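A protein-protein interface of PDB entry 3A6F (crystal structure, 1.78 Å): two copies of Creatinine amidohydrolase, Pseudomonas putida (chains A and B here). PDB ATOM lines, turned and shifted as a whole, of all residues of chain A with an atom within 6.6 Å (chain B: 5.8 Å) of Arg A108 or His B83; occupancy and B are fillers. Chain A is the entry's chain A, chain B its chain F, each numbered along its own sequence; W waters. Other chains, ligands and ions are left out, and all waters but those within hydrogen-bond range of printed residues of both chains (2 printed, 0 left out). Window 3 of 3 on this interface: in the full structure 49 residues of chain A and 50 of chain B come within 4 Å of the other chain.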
ATOM      1  N   ILE A 103      28.937  31.548  14.224  1.00  0.00           N
ATOM      2  CA  ILE A 103      28.118  32.035  15.340  1.00  0.00           C
ATOM      3  C   ILE A 103      27.082  30.989  15.740  1.00  0.00           C
ATOM      4  O   ILE A 103      26.822  30.779  16.929  1.00  0.00           O
ATOM      5  CB  ILE A 103      27.409  33.370  14.978  1.00  0.00           C
ATOM      6  CG1 ILE A 103      28.463  34.465  14.794  1.00  0.00           C
ATOM      7  CG2 ILE A 103      26.412  33.758  16.079  1.00  0.00           C
ATOM      8  CD1 ILE A 103      27.923  35.774  14.220  1.00  0.00           C
ATOM      9  N   ARG A 104      26.498  30.319  14.754  1.00  0.00           N
ATOM     10  CA  ARG A 104      25.507  29.288  15.031  1.00  0.00           C
ATOM     11  C   ARG A 104      26.171  28.189  15.872  1.00  0.00           C
ATOM     12  O   ARG A 104      25.585  27.675  16.825  1.00  0.00           O
ATOM     13  CB  ARG A 104      24.982  28.680  13.718  1.00  0.00           C
ATOM     14  CG  ARG A 104      23.773  27.771  13.898  1.00  0.00           C
ATOM     15  CD  ARG A 104      23.395  26.987  12.618  1.00  0.00           C
ATOM     16  NE  ARG A 104      22.952  27.846  11.524  1.00  0.00           N
ATOM     17  CZ  ARG A 104      23.650  28.055  10.412  1.00  0.00           C
ATOM     18  NH1 ARG A 104      23.180  28.856   9.467  1.00  0.00           N
ATOM     19  NH2 ARG A 104      24.819  27.458  10.242  1.00  0.00           N
ATOM     20  N   GLU A 105      27.402  27.842  15.519  1.00  0.00           N
ATOM     21  CA  GLU A 105      28.124  26.792  16.239  1.00  0.00           C
ATOM     22  C   GLU A 105      28.556  27.212  17.647  1.00  0.00           C
ATOM     23  O   GLU A 105      28.449  26.428  18.597  1.00  0.00           O
ATOM     24  CB  GLU A 105      29.322  26.341  15.404  1.00  0.00           C
ATOM     25  CG  GLU A 105      28.896  25.519  14.179  1.00  0.00           C
ATOM     26  CD  GLU A 105      28.588  24.076  14.535  1.00  0.00           C
ATOM     27  OE1 GLU A 105      29.538  23.276  14.553  1.00  0.00           O
ATOM     28  OE2 GLU A 105      27.407  23.742  14.813  1.00  0.00           O
ATOM     29  N   LEU A 106      29.042  28.442  17.787  1.00  0.00           N
ATOM     30  CA  LEU A 106      29.454  28.929  19.100  1.00  0.00           C
ATOM     31  C   LEU A 106      28.251  28.897  20.044  1.00  0.00           C
ATOM     32  O   LEU A 106      28.374  28.491  21.204  1.00  0.00           O
ATOM     33  CB  LEU A 106      30.019  30.344  18.995  1.00  0.00           C
ATOM     34  CG  LEU A 106      31.356  30.443  18.245  1.00  0.00           C
ATOM     35  CD1 LEU A 106      31.843  31.889  18.243  1.00  0.00           C
ATOM     36  CD2 LEU A 106      32.386  29.527  18.908  1.00  0.00           C
ATOM     37  N   ALA A 107      27.090  29.314  19.543  1.00  0.00           N
ATOM     38  CA  ALA A 107      25.867  29.302  20.347  1.00  0.00           C
ATOM     39  C   ALA A 107      25.554  27.882  20.801  1.00  0.00           C
ATOM     40  O   ALA A 107      25.170  27.657  21.958  1.00  0.00           O
ATOM     41  CB  ALA A 107      24.703  29.865  19.543  1.00  0.00           C
ATOM     42  N   ARG A 108      25.698  26.926  19.886  1.00  0.00           N
ATOM     43  CA  ARG A 108      25.466  25.523  20.201  1.00  0.00           C
ATOM     44  C   ARG A 108      26.399  25.085  21.333  1.00  0.00           C
ATOM     45  O   ARG A 108      25.994  24.338  22.219  1.00  0.00           O
ATOM     46  CB  ARG A 108      25.704  24.641  18.962  1.00  0.00           C
ATOM     47  CG  ARG A 108      25.662  23.139  19.261  1.00  0.00           C
ATOM     48  CD  ARG A 108      25.817  22.287  17.996  1.00  0.00           C
ATOM     49  NE  ARG A 108      27.135  22.446  17.374  1.00  0.00           N
ATOM     50  CZ  ARG A 108      28.274  21.985  17.883  1.00  0.00           C
ATOM     51  NH1 ARG A 108      28.278  21.322  19.041  1.00  0.00           N
ATOM     52  NH2 ARG A 108      29.416  22.187  17.231  1.00  0.00           N
ATOM     53  N   HIS A 109      27.647  25.554  21.302  1.00  0.00           N
ATOM     54  CA  HIS A 109      28.622  25.211  22.336  1.00  0.00           C
ATOM     55  C   HIS A 109      28.189  25.743  23.697  1.00  0.00           C
ATOM     56  O   HIS A 109      28.536  25.176  24.738  1.00  0.00           O
ATOM     57  CB  HIS A 109      29.987  25.816  22.029  1.00  0.00           C
ATOM     58  CG  HIS A 109      30.588  25.358  20.739  1.00  0.00           C
ATOM     59  ND1 HIS A 109      31.740  25.917  20.228  1.00  0.00           N
ATOM     60  CD2 HIS A 109      30.226  24.380  19.873  1.00  0.00           C
ATOM     61  CE1 HIS A 109      32.064  25.301  19.104  1.00  0.00           C
ATOM     62  NE2 HIS A 109      31.163  24.366  18.866  1.00  0.00           N
ATOM     63  N   GLY A 110      27.437  26.838  23.685  1.00  0.00           N
ATOM     64  CA  GLY A 110      26.998  27.435  24.931  1.00  0.00           C
ATOM     65  C   GLY A 110      27.699  28.762  25.155  1.00  0.00           C
ATOM     66  O   GLY A 110      27.523  29.401  26.190  1.00  0.00           O
ATOM     67  N   ALA A 111      28.513  29.175  24.187  1.00  0.00           N
ATOM     68  CA  ALA A 111      29.213  30.452  24.280  1.00  0.00           C
ATOM     69  C   ALA A 111      28.171  31.525  23.965  1.00  0.00           C
ATOM     70  O   ALA A 111      27.230  31.271  23.216  1.00  0.00           O
ATOM     71  CB  ALA A 111      30.356  30.502  23.276  1.00  0.00           C
ATOM     72  N   ARG A 112      28.335  32.717  24.535  1.00  0.00           N
ATOM     73  CA  ARG A 112      27.368  33.791  24.319  1.00  0.00           C
ATOM     74  C   ARG A 112      28.016  35.162  24.150  1.00  0.00           C
ATOM     75  O   ARG A 112      27.322  36.179  24.095  1.00  0.00           O
ATOM     76  CB  ARG A 112      26.393  33.839  25.504  1.00  0.00           C
ATOM     77  CG  ARG A 112      25.512  32.609  25.651  1.00  0.00           C
ATOM     78  CD  ARG A 112      24.397  32.632  24.619  1.00  0.00           C
ATOM     79  NE  ARG A 112      23.424  31.558  24.798  1.00  0.00           N
ATOM     80  CZ  ARG A 112      23.588  30.305  24.381  1.00  0.00           C
ATOM     81  NH1 ARG A 112      24.702  29.936  23.750  1.00  0.00           N
ATOM     82  NH2 ARG A 112      22.618  29.425  24.569  1.00  0.00           N
ATOM     83  N   LEU A 138      19.279  32.198  15.936  1.00  0.00           N
ATOM     84  CA  LEU A 138      19.396  31.913  17.362  1.00  0.00           C
ATOM     85  C   LEU A 138      18.060  32.198  18.029  1.00  0.00           C
ATOM     86  O   LEU A 138      17.614  31.444  18.887  1.00  0.00           O
ATOM     87  CB  LEU A 138      20.494  32.767  18.009  1.00  0.00           C
ATOM     88  CG  LEU A 138      21.933  32.543  17.528  1.00  0.00           C
ATOM     89  CD1 LEU A 138      22.897  33.227  18.490  1.00  0.00           C
ATOM     90  CD2 LEU A 138      22.233  31.064  17.440  1.00  0.00           C
ATOM     91  N   ILE A 143      17.291  31.395  21.640  1.00  0.00           N
ATOM     92  CA  ILE A 143      18.454  32.041  22.234  1.00  0.00           C
ATOM     93  C   ILE A 143      18.458  33.537  21.952  1.00  0.00           C
ATOM     94  O   ILE A 143      18.497  33.958  20.797  1.00  0.00           O
ATOM     95  CB  ILE A 143      19.758  31.430  21.683  1.00  0.00           C
ATOM     96  CG1 ILE A 143      19.795  29.928  21.987  1.00  0.00           C
ATOM     97  CG2 ILE A 143      20.967  32.141  22.285  1.00  0.00           C
ATOM     98  CD1 ILE A 143      20.940  29.194  21.303  1.00  0.00           C
ATOM     99  N   PHE A 146      22.895  36.012  23.290  1.00  0.00           N
ATOM    100  CA  PHE A 146      24.192  35.960  22.612  1.00  0.00           C
ATOM    101  C   PHE A 146      24.507  37.398  22.206  1.00  0.00           C
ATOM    102  O   PHE A 146      23.721  38.026  21.503  1.00  0.00           O
ATOM    103  CB  PHE A 146      24.099  35.060  21.367  1.00  0.00           C
ATOM    104  CG  PHE A 146      25.436  34.652  20.804  1.00  0.00           C
ATOM    105  CD1 PHE A 146      26.204  35.546  20.074  1.00  0.00           C
ATOM    106  CD2 PHE A 146      25.935  33.367  21.031  1.00  0.00           C
ATOM    107  CE1 PHE A 146      27.462  35.175  19.576  1.00  0.00           C
ATOM    108  CE2 PHE A 146      27.189  32.984  20.540  1.00  0.00           C
ATOM    109  CZ  PHE A 146      27.952  33.891  19.813  1.00  0.00           C
ATOM    110  N   GLN B  76      29.476  11.299  12.917  1.00  0.00           N
ATOM    111  CA  GLN B  76      29.715  10.315  13.969  1.00  0.00           C
ATOM    112  C   GLN B  76      30.716   9.208  13.665  1.00  0.00           C
ATOM    113  O   GLN B  76      31.633   8.968  14.451  1.00  0.00           O
ATOM    114  CB  GLN B  76      28.389   9.686  14.403  1.00  0.00           C
ATOM    115  CG  GLN B  76      28.533   8.660  15.526  1.00  0.00           C
ATOM    116  CD  GLN B  76      27.258   8.521  16.324  1.00  0.00           C
ATOM    117  OE1 GLN B  76      26.230   8.083  15.803  1.00  0.00           O
ATOM    118  NE2 GLN B  76      27.308   8.914  17.593  1.00  0.00           N
ATOM    119  N   GLY B  80      33.360  11.669  15.113  1.00  0.00           N
ATOM    120  CA  GLY B  80      32.755  11.673  16.434  1.00  0.00           C
ATOM    121  C   GLY B  80      31.347  12.236  16.480  1.00  0.00           C
ATOM    122  O   GLY B  80      30.526  11.778  17.269  1.00  0.00           O
ATOM    123  N   GLY B  81      31.069  13.243  15.652  1.00  0.00           N
ATOM    124  CA  GLY B  81      29.745  13.841  15.636  1.00  0.00           C
ATOM    125  C   GLY B  81      29.803  15.338  15.877  1.00  0.00           C
ATOM    126  O   GLY B  81      30.708  15.834  16.553  1.00  0.00           O
ATOM    127  N   ASN B  82      28.827  16.066  15.347  1.00  0.00           N
ATOM    128  CA  ASN B  82      28.825  17.511  15.493  1.00  0.00           C
ATOM    129  C   ASN B  82      28.132  18.005  16.759  1.00  0.00           C
ATOM    130  O   ASN B  82      27.722  19.165  16.837  1.00  0.00           O
ATOM    131  CB  ASN B  82      28.192  18.166  14.259  1.00  0.00           C
ATOM    132  CG  ASN B  82      28.848  19.489  13.909  1.00  0.00           C
ATOM    133  OD1 ASN B  82      29.990  19.526  13.439  1.00  0.00           O
ATOM    134  ND2 ASN B  82      28.141  20.583  14.152  1.00  0.00           N
ATOM    135  N   HIS B  83      28.018  17.131  17.753  1.00  0.00           N
ATOM    136  CA  HIS B  83      27.392  17.503  19.013  1.00  0.00           C
ATOM    137  C   HIS B  83      28.444  17.891  20.048  1.00  0.00           C
ATOM    138  O   HIS B  83      28.115  18.376  21.133  1.00  0.00           O
ATOM    139  CB  HIS B  83      26.538  16.353  19.549  1.00  0.00           C
ATOM    140  CG  HIS B  83      27.307  15.095  19.809  1.00  0.00           C
ATOM    141  ND1 HIS B  83      27.926  14.378  18.806  1.00  0.00           N
ATOM    142  CD2 HIS B  83      27.564  14.429  20.961  1.00  0.00           C
ATOM    143  CE1 HIS B  83      28.530  13.326  19.330  1.00  0.00           C
ATOM    144  NE2 HIS B  83      28.325  13.333  20.636  1.00  0.00           N
ATOM    145  N   PHE B  84      29.713  17.677  19.716  1.00  0.00           N
ATOM    146  CA  PHE B  84      30.784  18.022  20.638  1.00  0.00           C
ATOM    147  C   PHE B  84      31.048  19.517  20.659  1.00  0.00           C
ATOM    148  O   PHE B  84      30.911  20.209  19.648  1.00  0.00           O
ATOM    149  CB  PHE B  84      32.102  17.325  20.265  1.00  0.00           C
ATOM    150  CG  PHE B  84      32.159  15.861  20.621  1.00  0.00           C
ATOM    151  CD1 PHE B  84      31.676  14.894  19.743  1.00  0.00           C
ATOM    152  CD2 PHE B  84      32.721  15.452  21.827  1.00  0.00           C
ATOM    153  CE1 PHE B  84      31.756  13.539  20.061  1.00  0.00           C
ATOM    154  CE2 PHE B  84      32.805  14.100  22.160  1.00  0.00           C
ATOM    155  CZ  PHE B  84      32.322  13.140  21.272  1.00  0.00           C
ATOM    156  N   PRO B  85      31.405  20.046  21.833  1.00  0.00           N
ATOM    157  CA  PRO B  85      31.690  21.476  21.892  1.00  0.00           C
ATOM    158  C   PRO B  85      33.073  21.632  21.240  1.00  0.00           C
ATOM    159  O   PRO B  85      33.788  20.645  21.074  1.00  0.00           O
ATOM    160  CB  PRO B  85      31.694  21.764  23.393  1.00  0.00           C
ATOM    161  CG  PRO B  85      32.133  20.466  24.001  1.00  0.00           C
ATOM    162  CD  PRO B  85      31.417  19.426  23.171  1.00  0.00           C
ATOM    163  N   GLY B  86      33.436  22.846  20.840  1.00  0.00           N
ATOM    164  CA  GLY B  86      34.739  23.037  20.219  1.00  0.00           C
ATOM    165  C   GLY B  86      34.660  22.871  18.717  1.00  0.00           C
ATOM    166  O   GLY B  86      35.065  23.759  17.969  1.00  0.00           O
ATOM    167  N   THR B  87      34.149  21.727  18.272  1.00  0.00           N
ATOM    168  CA  THR B  87      33.982  21.490  16.847  1.00  0.00           C
ATOM    169  C   THR B  87      33.097  22.619  16.309  1.00  0.00           C
ATOM    170  O   THR B  87      31.981  22.826  16.781  1.00  0.00           O
ATOM    171  CB  THR B  87      33.311  20.143  16.597  1.00  0.00           C
ATOM    172  OG1 THR B  87      34.144  19.101  17.126  1.00  0.00           O
ATOM    173  CG2 THR B  87      33.084  19.922  15.098  1.00  0.00           C
ATOM    174  N   THR B  88      33.597  23.340  15.314  1.00  0.00           N
ATOM    175  CA  THR B  88      32.874  24.480  14.742  1.00  0.00           C
ATOM    176  C   THR B  88      32.818  24.254  13.238  1.00  0.00           C
ATOM    177  O   THR B  88      33.801  24.476  12.531  1.00  0.00           O
ATOM    178  CB  THR B  88      33.628  25.776  15.084  1.00  0.00           C
ATOM    179  OG1 THR B  88      33.794  25.847  16.508  1.00  0.00           O
ATOM    180  CG2 THR B  88      32.863  27.000  14.610  1.00  0.00           C
ATOM    181  N   SER B  89      31.660  23.802  12.765  1.00  0.00           N
ATOM    182  CA  SER B  89      31.477  23.447  11.359  1.00  0.00           C
ATOM    183  C   SER B  89      30.650  24.371  10.475  1.00  0.00           C
ATOM    184  O   SER B  89      29.737  25.049  10.936  1.00  0.00           O
ATOM    185  CB  SER B  89      30.867  22.051  11.281  1.00  0.00           C
ATOM    186  OG  SER B  89      31.537  21.148  12.147  1.00  0.00           O
ATOM    187  N   VAL B 216      22.230  13.002  15.713  1.00  0.00           N
ATOM    188  CA  VAL B 216      23.325  12.183  16.209  1.00  0.00           C
ATOM    189  C   VAL B 216      23.074  11.771  17.662  1.00  0.00           C
ATOM    190  O   VAL B 216      22.686  12.588  18.491  1.00  0.00           O
ATOM    191  CB  VAL B 216      24.692  12.925  16.080  1.00  0.00           C
ATOM    192  CG1 VAL B 216      24.660  14.248  16.838  1.00  0.00           C
ATOM    193  CG2 VAL B 216      25.820  12.032  16.597  1.00  0.00           C
ATOM    194  N   ASP B 217      23.270  10.484  17.946  1.00  0.00           N
ATOM    195  CA  ASP B 217      23.076   9.934  19.287  1.00  0.00           C
ATOM    196  C   ASP B 217      24.433   9.894  19.995  1.00  0.00           C
ATOM    197  O   ASP B 217      25.280   9.062  19.678  1.00  0.00           O
ATOM    198  CB  ASP B 217      22.492   8.524  19.180  1.00  0.00           C
ATOM    199  CG  ASP B 217      22.288   7.861  20.537  1.00  0.00           C
ATOM    200  OD1 ASP B 217      22.551   8.508  21.575  1.00  0.00           O
ATOM    201  OD2 ASP B 217      21.860   6.688  20.557  1.00  0.00           O
ATOM    202  N   PRO B 218      24.649  10.798  20.969  1.00  0.00           N
ATOM    203  CA  PRO B 218      25.901  10.887  21.730  1.00  0.00           C
ATOM    204  C   PRO B 218      26.357   9.563  22.342  1.00  0.00           C
ATOM    205  O   PRO B 218      27.553   9.344  22.558  1.00  0.00           O
ATOM    206  CB  PRO B 218      25.584  11.933  22.798  1.00  0.00           C
ATOM    207  CG  PRO B 218      24.549  12.807  22.131  1.00  0.00           C
ATOM    208  CD  PRO B 218      23.667  11.778  21.471  1.00  0.00           C
ATOM    209  N   THR B 221      29.088   7.343  20.357  1.00  0.00           N
ATOM    210  CA  THR B 221      30.460   7.792  20.146  1.00  0.00           C
ATOM    211  C   THR B 221      31.178   7.643  21.481  1.00  0.00           C
ATOM    212  O   THR B 221      30.602   7.940  22.527  1.00  0.00           O
ATOM    213  CB  THR B 221      30.536   9.284  19.724  1.00  0.00           C
ATOM    214  OG1 THR B 221      29.938   9.459  18.434  1.00  0.00           O
ATOM    215  CG2 THR B 221      31.988   9.738  19.659  1.00  0.00           C
HETATM  216  O   HOH W   1      27.002  24.827  10.462  1.00  0.00           O
HETATM  217  O   HOH W   2      26.068  20.227  20.897  1.00  0.00           O
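O of Phe B84 sits at hydrogen-bond distance from NH1 of Arg A108, at 2.9 Å. The backbone NH of Gly B86 lies close to a ring nitrogen (NE2) of His A109, 3.4 Å away. OE1 of Glu A105 sits close to O of Thr B87 (3.3 Å). The side-chain carboxylate (OE1) of Glu A105 lies within hydrogen-bond range of the backbone NH (N) of Ser B89 (2.8 Å). The guanidinium group of Arg A108 lies within hydrogen-bond range of the backbone carbonyl oxygen of Thr B87. The backbone carbonyl oxygen (O) of Asn B82 sits close to the guanidinium group (NH1) of Arg A108, at 3.1 Å. The side-chain amide nitrogen of Asn B82 sits at hydrogen-bond distance from the side-chain carboxylate of Glu A105, at 3.1 Å. O of Thr B87 sits at hydrogen-bond distance from NE2 of His A109, at 2.7 Å.
The guanidinium group (NH2) of Arg A108 sits at hydrogen-bond distance from a ring nitrogen (NE2) of His A109, at 3.2 Å. The side-chain carboxylate of Glu A105 lies within salt-bridge range of the guanidinium group of Arg A108 (2.9 Å). A ring nitrogen (NE2) of His A109 sits close to the backbone carbonyl oxygen (O) of Glu A105. The backbone carbonyl oxygen of Gly B86 sits at hydrogen-bond distance from the side-chain hydroxyl of Thr B88 (2.8 Å). The side-chain amide oxygen of Asn B82 is in hydrogen-bond range of the side-chain hydroxyl of Ser B89, at 2.6 Å.
OE1 of Glu A105 touches CA of Thr B88 (3.6 Å). C of His B83 touches NH1 of Arg A108, 3.6 Å away. Pro B85 touches His A109 (CA to CD2, 3.8 Å). OG1 of Thr B88 touches CE1 of His A109, at 3.2 Å.
Ile A103 touches none of the printed residues of chain B. Printed residues of chain B within 4 Å of Glu A105: Asn B82 (3.1 Å), Thr B87 (3.3 Å), Thr B88 (3.6 Å) and Ser B89 (2.8 Å). Of chain B, only Asn B82, His B83, Phe B84 and Thr B87 come within 4 Å of Arg A108. Of the printed residues of chain B, His A109 touches Pro B85 (3.8 Å), Gly B86 (3.3 Å), Thr B87 (2.7 Å) and Thr B88 (3.2 Å). His B83 touches just one residue of chain A: Arg A108. Printed residues of chain A within 4 Å of Thr B88: Glu A105 (3.6 Å) and His A109 (3.2 Å).
Of the 13 printed residues of chain A, 3 touch a printed residue of chain B. Among the printed residues, 12 pairs touch across the chains.
No position is printed for both chains. Of the 12 pairs that touch across the chains among the printed residues, none has its exchanged pair printed and touching as well.
Water W2 lies within hydrogen-bond range of O of His B83 and NH1 of Arg A108. Water W1 bridges the backbone carbonyl oxygen (O) of Ser B89 (2.8 Å) and the guanidinium group (NH2) of Arg A104 (3.4 Å).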
